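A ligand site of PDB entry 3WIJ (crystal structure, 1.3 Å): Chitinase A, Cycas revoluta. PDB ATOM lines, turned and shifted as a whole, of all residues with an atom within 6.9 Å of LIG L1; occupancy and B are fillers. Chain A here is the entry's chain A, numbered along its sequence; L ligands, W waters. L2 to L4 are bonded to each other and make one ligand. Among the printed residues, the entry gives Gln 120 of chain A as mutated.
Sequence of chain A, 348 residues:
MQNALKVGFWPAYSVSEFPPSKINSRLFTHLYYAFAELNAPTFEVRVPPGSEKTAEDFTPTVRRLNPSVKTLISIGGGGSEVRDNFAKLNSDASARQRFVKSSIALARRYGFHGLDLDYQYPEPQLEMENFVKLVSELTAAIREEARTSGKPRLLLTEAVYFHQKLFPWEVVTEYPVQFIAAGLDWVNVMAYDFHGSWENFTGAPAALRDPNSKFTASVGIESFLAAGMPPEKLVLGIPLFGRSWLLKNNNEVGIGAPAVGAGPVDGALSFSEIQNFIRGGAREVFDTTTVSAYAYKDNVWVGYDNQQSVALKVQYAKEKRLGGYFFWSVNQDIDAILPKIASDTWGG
O3 of LIG L1 is in hydrogen-bond range of O of Glu 170, at 2.9 Å. OE2 of Glu 170 lies close to O2 of LIG L1, at 3.3 Å. OE1 of Glu 123 is in hydrogen-bond range of O1 of LIG L1 (3.4 Å). An oxygen (O5) of LG3 L3 is in hydrogen-bond range of the side-chain hydroxyl (OH) of Tyr 161 (2.6 Å). NE1 of Trp 198 sits at hydrogen-bond distance from O5 of LG2 L2 (3.1 Å).
An oxygen (O5) of LIG L1 sits at hydrogen-bond distance from an oxygen (O3) of LG2 L2 (2.8 Å).
The backbone NH of Val 172 is in hydrogen-bond range of the backbone carbonyl oxygen of Leu 166.
Merely in contact with LIG L1: Trp 169, Phe 167, Tyr 121 and Val 172. Within 4 Å of LIG L1: Tyr 121, Glu 123, Phe 167, Trp 169, Glu 170 and Val 172. The nearest printed residue that does not touch LIG L1 is Tyr 161 (4.3 Å).
Water W4 lies within hydrogen-bond range of OE2 of Glu 123 (2.5 Å) and O4 of LIG L1 (2.7 Å). Water W2 bridges a nitrogen (N2) of LIG L1 and the indole nitrogen of Trp 169. Water W3 bridges O2 of LG2 L2 and N1 of LIG L1.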
ATOM      1  N   ARG A  83      14.894   6.252 -24.407  1.00  0.00           N
ATOM      2  CA  ARG A  83      15.694   6.780 -23.291  1.00  0.00           C
ATOM      3  C   ARG A  83      15.081   6.363 -21.941  1.00  0.00           C
ATOM      4  O   ARG A  83      15.791   5.954 -21.015  1.00  0.00           O
ATOM      5  CB  ARG A  83      15.783   8.308 -23.405  1.00  0.00           C
ATOM      6  CG  ARG A  83      16.518   8.980 -22.250  1.00  0.00           C
ATOM      7  CD  ARG A  83      16.095  10.427 -22.096  1.00  0.00           C
ATOM      8  NE  ARG A  83      14.683  10.513 -21.739  1.00  0.00           N
ATOM      9  CZ  ARG A  83      13.875  11.533 -22.057  1.00  0.00           C
ATOM     10  NH1 ARG A  83      14.324  12.565 -22.762  1.00  0.00           N
ATOM     11  NH2 ARG A  83      12.611  11.484 -21.684  1.00  0.00           N
ATOM     12  N   GLN A 120      20.057   7.778 -26.216  1.00  0.00           N
ATOM     13  CA  GLN A 120      20.199   9.227 -26.283  1.00  0.00           C
ATOM     14  C   GLN A 120      19.417   9.852 -25.148  1.00  0.00           C
ATOM     15  O   GLN A 120      18.238  10.150 -25.325  1.00  0.00           O
ATOM     16  CB  GLN A 120      19.723   9.733 -27.642  1.00  0.00           C
ATOM     17  CG  GLN A 120      20.539   9.111 -28.787  1.00  0.00           C
ATOM     18  CD  GLN A 120      20.185   9.620 -30.155  1.00  0.00           C
ATOM     19  OE1 GLN A 120      19.791  10.766 -30.319  1.00  0.00           O
ATOM     20  NE2 GLN A 120      20.355   8.785 -31.163  1.00  0.00           N
ATOM     21  N   TYR A 121      20.024  10.091 -23.982  1.00  0.00           N
ATOM     22  CA  TYR A 121      21.473   9.951 -23.698  1.00  0.00           C
ATOM     23  C   TYR A 121      21.644   9.483 -22.247  1.00  0.00           C
ATOM     24  O   TYR A 121      20.743   9.691 -21.429  1.00  0.00           O
ATOM     25  CB  TYR A 121      22.182  11.302 -23.814  1.00  0.00           C
ATOM     26  CG  TYR A 121      22.097  11.867 -25.208  1.00  0.00           C
ATOM     27  CD1 TYR A 121      23.019  11.496 -26.204  1.00  0.00           C
ATOM     28  CD2 TYR A 121      21.101  12.773 -25.539  1.00  0.00           C
ATOM     29  CE1 TYR A 121      22.917  12.028 -27.487  1.00  0.00           C
ATOM     30  CE2 TYR A 121      20.992  13.287 -26.811  1.00  0.00           C
ATOM     31  CZ  TYR A 121      21.893  12.918 -27.769  1.00  0.00           C
ATOM     32  OH  TYR A 121      21.781  13.473 -29.038  1.00  0.00           O
ATOM     33  N   GLU A 123      22.482  10.473 -19.374  1.00  0.00           N
ATOM     34  CA  GLU A 123      22.679  11.629 -18.509  1.00  0.00           C
ATOM     35  C   GLU A 123      21.390  11.794 -17.721  1.00  0.00           C
ATOM     36  O   GLU A 123      20.320  11.445 -18.219  1.00  0.00           O
ATOM     37  CB  GLU A 123      23.020  12.895 -19.332  1.00  0.00           C
ATOM     38  CG  GLU A 123      21.951  13.347 -20.336  1.00  0.00           C
ATOM     39  CD  GLU A 123      20.898  14.251 -19.721  1.00  0.00           C
ATOM     40  OE1 GLU A 123      21.108  14.732 -18.594  1.00  0.00           O
ATOM     41  OE2 GLU A 123      19.867  14.479 -20.389  1.00  0.00           O
ATOM     42  N   PRO A 124      21.457  12.352 -16.516  1.00  0.00           N
ATOM     43  CA  PRO A 124      22.610  12.899 -15.815  1.00  0.00           C
ATOM     44  C   PRO A 124      23.513  11.833 -15.182  1.00  0.00           C
ATOM     45  O   PRO A 124      23.529  10.670 -15.631  1.00  0.00           O
ATOM     46  CB  PRO A 124      21.964  13.841 -14.786  1.00  0.00           C
ATOM     47  CG  PRO A 124      20.682  13.206 -14.493  1.00  0.00           C
ATOM     48  CD  PRO A 124      20.194  12.612 -15.791  1.00  0.00           C
ATOM     49  N   TYR A 161      26.866  11.068 -28.447  1.00  0.00           N
ATOM     50  CA  TYR A 161      26.703  12.477 -28.747  1.00  0.00           C
ATOM     51  C   TYR A 161      27.958  12.998 -29.478  1.00  0.00           C
ATOM     52  O   TYR A 161      29.041  12.406 -29.376  1.00  0.00           O
ATOM     53  CB  TYR A 161      26.519  13.199 -27.433  1.00  0.00           C
ATOM     54  CG  TYR A 161      26.112  14.655 -27.491  1.00  0.00           C
ATOM     55  CD1 TYR A 161      26.893  15.638 -26.882  1.00  0.00           C
ATOM     56  CD2 TYR A 161      24.929  15.053 -28.134  1.00  0.00           C
ATOM     57  CE1 TYR A 161      26.523  16.967 -26.911  1.00  0.00           C
ATOM     58  CE2 TYR A 161      24.552  16.401 -28.170  1.00  0.00           C
ATOM     59  CZ  TYR A 161      25.346  17.332 -27.540  1.00  0.00           C
ATOM     60  OH  TYR A 161      25.019  18.680 -27.543  1.00  0.00           O
ATOM     61  N   LEU A 166      28.482  15.699 -21.745  1.00  0.00           N
ATOM     62  CA  LEU A 166      27.044  15.867 -21.772  1.00  0.00           C
ATOM     63  C   LEU A 166      26.693  16.902 -20.724  1.00  0.00           C
ATOM     64  O   LEU A 166      26.590  16.556 -19.546  1.00  0.00           O
ATOM     65  CB  LEU A 166      26.331  14.527 -21.468  1.00  0.00           C
ATOM     66  CG  LEU A 166      26.619  13.390 -22.452  1.00  0.00           C
ATOM     67  CD1 LEU A 166      26.006  12.095 -21.955  1.00  0.00           C
ATOM     68  CD2 LEU A 166      26.042  13.711 -23.823  1.00  0.00           C
ATOM     69  N   PHE A 167      26.533  18.172 -21.085  1.00  0.00           N
ATOM     70  CA  PHE A 167      26.654  18.737 -22.428  1.00  0.00           C
ATOM     71  C   PHE A 167      27.673  19.865 -22.367  1.00  0.00           C
ATOM     72  O   PHE A 167      27.966  20.363 -21.270  1.00  0.00           O
ATOM     73  CB  PHE A 167      25.265  19.220 -22.879  1.00  0.00           C
ATOM     74  CG  PHE A 167      24.286  18.083 -23.024  1.00  0.00           C
ATOM     75  CD1 PHE A 167      23.509  17.642 -21.940  1.00  0.00           C
ATOM     76  CD2 PHE A 167      24.207  17.401 -24.224  1.00  0.00           C
ATOM     77  CE1 PHE A 167      22.641  16.539 -22.095  1.00  0.00           C
ATOM     78  CE2 PHE A 167      23.355  16.288 -24.367  1.00  0.00           C
ATOM     79  CZ  PHE A 167      22.583  15.861 -23.302  1.00  0.00           C
ATOM     80  N   PRO A 168      28.248  20.250 -23.522  1.00  0.00           N
ATOM     81  CA  PRO A 168      29.352  21.219 -23.464  1.00  0.00           C
ATOM     82  C   PRO A 168      29.056  22.538 -22.757  1.00  0.00           C
ATOM     83  O   PRO A 168      29.964  23.086 -22.121  1.00  0.00           O
ATOM     84  CB  PRO A 168      29.701  21.471 -24.919  1.00  0.00           C
ATOM     85  CG  PRO A 168      28.845  20.616 -25.752  1.00  0.00           C
ATOM     86  CD  PRO A 168      28.036  19.725 -24.888  1.00  0.00           C
ATOM     87  N   TRP A 169      27.818  23.025 -22.851  1.00  0.00           N
ATOM     88  CA  TRP A 169      27.431  24.296 -22.213  1.00  0.00           C
ATOM     89  C   TRP A 169      27.086  24.144 -20.715  1.00  0.00           C
ATOM     90  O   TRP A 169      26.991  25.138 -19.995  1.00  0.00           O
ATOM     91  CB  TRP A 169      26.263  24.922 -22.968  1.00  0.00           C
ATOM     92  CG  TRP A 169      24.991  24.108 -22.934  1.00  0.00           C
ATOM     93  CD1 TRP A 169      23.991  24.180 -21.992  1.00  0.00           C
ATOM     94  CD2 TRP A 169      24.592  23.095 -23.862  1.00  0.00           C
ATOM     95  NE1 TRP A 169      22.998  23.276 -22.290  1.00  0.00           N
ATOM     96  CE2 TRP A 169      23.337  22.600 -23.438  1.00  0.00           C
ATOM     97  CE3 TRP A 169      25.167  22.574 -25.029  1.00  0.00           C
ATOM     98  CZ2 TRP A 169      22.656  21.598 -24.120  1.00  0.00           C
ATOM     99  CZ3 TRP A 169      24.486  21.572 -25.710  1.00  0.00           C
ATOM    100  CH2 TRP A 169      23.246  21.099 -25.256  1.00  0.00           C
ATOM    101  N   GLU A 170      26.891  22.905 -20.259  1.00  0.00           N
ATOM    102  CA  GLU A 170      26.547  22.629 -18.872  1.00  0.00           C
ATOM    103  C   GLU A 170      26.812  21.147 -18.642  1.00  0.00           C
ATOM    104  O   GLU A 170      25.990  20.298 -18.986  1.00  0.00           O
ATOM    105  CB  GLU A 170      25.099  23.001 -18.586  1.00  0.00           C
ATOM    106  CG  GLU A 170      24.662  22.808 -17.125  1.00  0.00           C
ATOM    107  CD  GLU A 170      23.340  23.475 -16.829  1.00  0.00           C
ATOM    108  OE1 GLU A 170      23.072  23.775 -15.645  1.00  0.00           O
ATOM    109  OE2 GLU A 170      22.557  23.708 -17.778  1.00  0.00           O
ATOM    110  N   VAL A 171      27.990  20.857 -18.117  1.00  0.00           N
ATOM    111  CA  VAL A 171      28.460  19.490 -18.003  1.00  0.00           C
ATOM    112  C   VAL A 171      27.822  18.803 -16.791  1.00  0.00           C
ATOM    113  O   VAL A 171      28.036  19.222 -15.648  1.00  0.00           O
ATOM    114  CB  VAL A 171      30.006  19.411 -17.920  1.00  0.00           C
ATOM    115  CG1 VAL A 171      30.446  17.939 -17.829  1.00  0.00           C
ATOM    116  CG2 VAL A 171      30.674  20.099 -19.129  1.00  0.00           C
ATOM    117  N   VAL A 172      27.028  17.777 -17.047  1.00  0.00           N
ATOM    118  CA  VAL A 172      26.403  16.999 -15.976  1.00  0.00           C
ATOM    119  C   VAL A 172      27.041  15.626 -15.857  1.00  0.00           C
ATOM    120  O   VAL A 172      27.042  15.018 -14.784  1.00  0.00           O
ATOM    121  CB  VAL A 172      24.856  16.919 -16.131  1.00  0.00           C
ATOM    122  CG1 VAL A 172      24.278  18.320 -16.256  1.00  0.00           C
ATOM    123  CG2 VAL A 172      24.424  16.069 -17.310  1.00  0.00           C
ATOM    124  N   TRP A 198      14.560  24.443 -34.726  1.00  0.00           N
ATOM    125  CA  TRP A 198      14.421  24.965 -33.373  1.00  0.00           C
ATOM    126  C   TRP A 198      15.024  26.368 -33.249  1.00  0.00           C
ATOM    127  O   TRP A 198      14.772  27.075 -32.263  1.00  0.00           O
ATOM    128  CB  TRP A 198      15.032  24.021 -32.339  1.00  0.00           C
ATOM    129  CG  TRP A 198      16.512  23.745 -32.520  1.00  0.00           C
ATOM    130  CD1 TRP A 198      17.552  24.409 -31.937  1.00  0.00           C
ATOM    131  CD2 TRP A 198      17.087  22.704 -33.315  1.00  0.00           C
ATOM    132  NE1 TRP A 198      18.749  23.839 -32.328  1.00  0.00           N
ATOM    133  CE2 TRP A 198      18.496  22.792 -33.163  1.00  0.00           C
ATOM    134  CE3 TRP A 198      16.561  21.695 -34.122  1.00  0.00           C
ATOM    135  CZ2 TRP A 198      19.379  21.902 -33.800  1.00  0.00           C
ATOM    136  CZ3 TRP A 198      17.444  20.806 -34.759  1.00  0.00           C
ATOM    137  CH2 TRP A 198      18.832  20.934 -34.588  1.00  0.00           C
ATOM    138  N   PHE A 215      29.577  24.103 -31.850  1.00  0.00           N
ATOM    139  CA  PHE A 215      28.786  22.976 -32.366  1.00  0.00           C
ATOM    140  C   PHE A 215      29.263  22.562 -33.752  1.00  0.00           C
ATOM    141  O   PHE A 215      28.637  22.891 -34.763  1.00  0.00           O
ATOM    142  CB  PHE A 215      27.298  23.325 -32.376  1.00  0.00           C
ATOM    143  CG  PHE A 215      26.752  23.527 -31.008  1.00  0.00           C
ATOM    144  CD1 PHE A 215      26.486  24.794 -30.523  1.00  0.00           C
ATOM    145  CD2 PHE A 215      26.547  22.423 -30.171  1.00  0.00           C
ATOM    146  CE1 PHE A 215      25.992  24.975 -29.215  1.00  0.00           C
ATOM    147  CE2 PHE A 215      26.065  22.598 -28.874  1.00  0.00           C
ATOM    148  CZ  PHE A 215      25.789  23.869 -28.399  1.00  0.00           C
HETATM  149  C1  LIG L   1      19.600  19.391 -22.297  1.00  0.00           C
HETATM  150  C2  LIG L   1      20.622  19.362 -21.164  1.00  0.00           C
HETATM  151  C3  LIG L   1      20.192  18.667 -23.495  1.00  0.00           C
HETATM  152  N1  LIG L   1      19.278  18.688 -24.628  1.00  0.00           N
HETATM  153  C4  LIG L   1      19.557  17.912 -25.839  1.00  0.00           C
HETATM  154  C5  LIG L   1      19.619  16.428 -25.500  1.00  0.00           C
HETATM  155  C6  LIG L   1      20.882  18.277 -26.502  1.00  0.00           C
HETATM  156  C7  LIG L   1      18.433  18.183 -26.845  1.00  0.00           C
HETATM  157  N2  LIG L   1      20.189  20.058 -19.957  1.00  0.00           N
HETATM  158  C8  LIG L   1      20.918  19.958 -18.695  1.00  0.00           C
HETATM  159  C9  LIG L   1      21.108  18.496 -18.308  1.00  0.00           C
HETATM  160  C10 LIG L   1      20.099  20.674 -17.616  1.00  0.00           C
HETATM  161  C11 LIG L   1      22.269  20.665 -18.789  1.00  0.00           C
HETATM  162  O1  LIG L   1      19.826  17.879 -18.239  1.00  0.00           O
HETATM  163  O2  LIG L   1      19.783  22.002 -18.056  1.00  0.00           O
HETATM  164  O3  LIG L   1      23.204  19.921 -19.565  1.00  0.00           O
HETATM  165  O4  LIG L   1      18.558  16.029 -24.626  1.00  0.00           O
HETATM  166  O5  LIG L   1      20.883  19.652 -26.906  1.00  0.00           O
HETATM  167  O6  LIG L   1      18.189  19.605 -26.939  1.00  0.00           O
HETATM  168  C1  LG2 L   2      22.355  24.855 -27.592  1.00  0.00           C
HETATM  169  C2  LG2 L   2      20.982  24.450 -27.079  1.00  0.00           C
HETATM  170  C3  LG2 L   2      20.669  23.010 -27.474  1.00  0.00           C
HETATM  171  C4  LG2 L   2      20.929  22.729 -28.961  1.00  0.00           C
HETATM  172  C5  LG2 L   2      22.321  23.244 -29.326  1.00  0.00           C
HETATM  173  C6  LG2 L   2      22.709  23.063 -30.801  1.00  0.00           C
HETATM  174  C7  LG2 L   2      20.412  25.566 -24.960  1.00  0.00           C
HETATM  175  C8  LG2 L   2      20.604  25.592 -23.476  1.00  0.00           C
HETATM  176  N1  LG2 L   2      20.935  24.535 -25.621  1.00  0.00           N
HETATM  177  O1  LG2 L   2      22.547  26.245 -27.450  1.00  0.00           O
HETATM  178  O2  LG2 L   2      19.363  22.636 -27.107  1.00  0.00           O
HETATM  179  O3  LG2 L   2      20.891  21.327 -29.124  1.00  0.00           O
HETATM  180  O4  LG2 L   2      22.449  24.618 -28.990  1.00  0.00           O
HETATM  181  O5  LG2 L   2      21.772  23.727 -31.621  1.00  0.00           O
HETATM  182  O6  LG2 L   2      19.782  26.461 -25.524  1.00  0.00           O
HETATM  183  C1  LG3 L   3      20.051  20.809 -30.155  1.00  0.00           C
HETATM  184  C2  LG3 L   3      20.560  19.388 -30.435  1.00  0.00           C
HETATM  185  C3  LG3 L   3      19.718  18.628 -31.464  1.00  0.00           C
HETATM  186  C4  LG3 L   3      18.236  18.726 -31.129  1.00  0.00           C
HETATM  187  C5  LG3 L   3      17.868  20.156 -30.731  1.00  0.00           C
HETATM  188  C6  LG3 L   3      16.427  20.252 -30.269  1.00  0.00           C
HETATM  189  C7  LG3 L   3      22.986  19.260 -30.162  1.00  0.00           C
HETATM  190  C8  LG3 L   3      24.336  19.226 -30.823  1.00  0.00           C
HETATM  191  N1  LG3 L   3      21.915  19.426 -30.927  1.00  0.00           N
HETATM  192  O1  LG3 L   3      20.195  17.272 -31.573  1.00  0.00           O
HETATM  193  O2  LG3 L   3      17.472  18.406 -32.285  1.00  0.00           O
HETATM  194  O3  LG3 L   3      18.720  20.720 -29.736  1.00  0.00           O
HETATM  195  O4  LG3 L   3      16.279  19.546 -29.057  1.00  0.00           O
HETATM  196  O5  LG3 L   3      22.862  19.123 -28.908  1.00  0.00           O
HETATM  197  C1  LG4 L   4      16.913  17.086 -32.233  1.00  0.00           C
HETATM  198  C2  LG4 L   4      15.912  16.947 -33.392  1.00  0.00           C
HETATM  199  C3  LG4 L   4      15.472  15.490 -33.577  1.00  0.00           C
HETATM  200  C4  LG4 L   4      16.695  14.567 -33.591  1.00  0.00           C
HETATM  201  C5  LG4 L   4      17.520  14.798 -32.340  1.00  0.00           C
HETATM  202  C6  LG4 L   4      18.751  13.893 -32.251  1.00  0.00           C
HETATM  203  C7  LG4 L   4      14.452  18.787 -34.086  1.00  0.00           C
HETATM  204  C8  LG4 L   4      13.382  19.747 -33.697  1.00  0.00           C
HETATM  205  N1  LG4 L   4      14.770  17.819 -33.205  1.00  0.00           N
HETATM  206  O1  LG4 L   4      14.782  15.325 -34.802  1.00  0.00           O
HETATM  207  O2  LG4 L   4      16.275  13.225 -33.733  1.00  0.00           O
HETATM  208  O3  LG4 L   4      17.953  16.139 -32.382  1.00  0.00           O
HETATM  209  O4  LG4 L   4      19.833  14.444 -32.987  1.00  0.00           O
HETATM  210  O5  LG4 L   4      15.013  18.905 -35.178  1.00  0.00           O
HETATM  211  O   HOH W   1      16.563  18.448 -23.769  1.00  0.00           O
HETATM  212  O   HOH W   2      20.201  22.549 -21.304  1.00  0.00           O
HETATM  213  O   HOH W   3      19.442  21.714 -24.622  1.00  0.00           O
HETATM  214  O   HOH W   4      19.509  14.229 -22.803  1.00  0.00           O
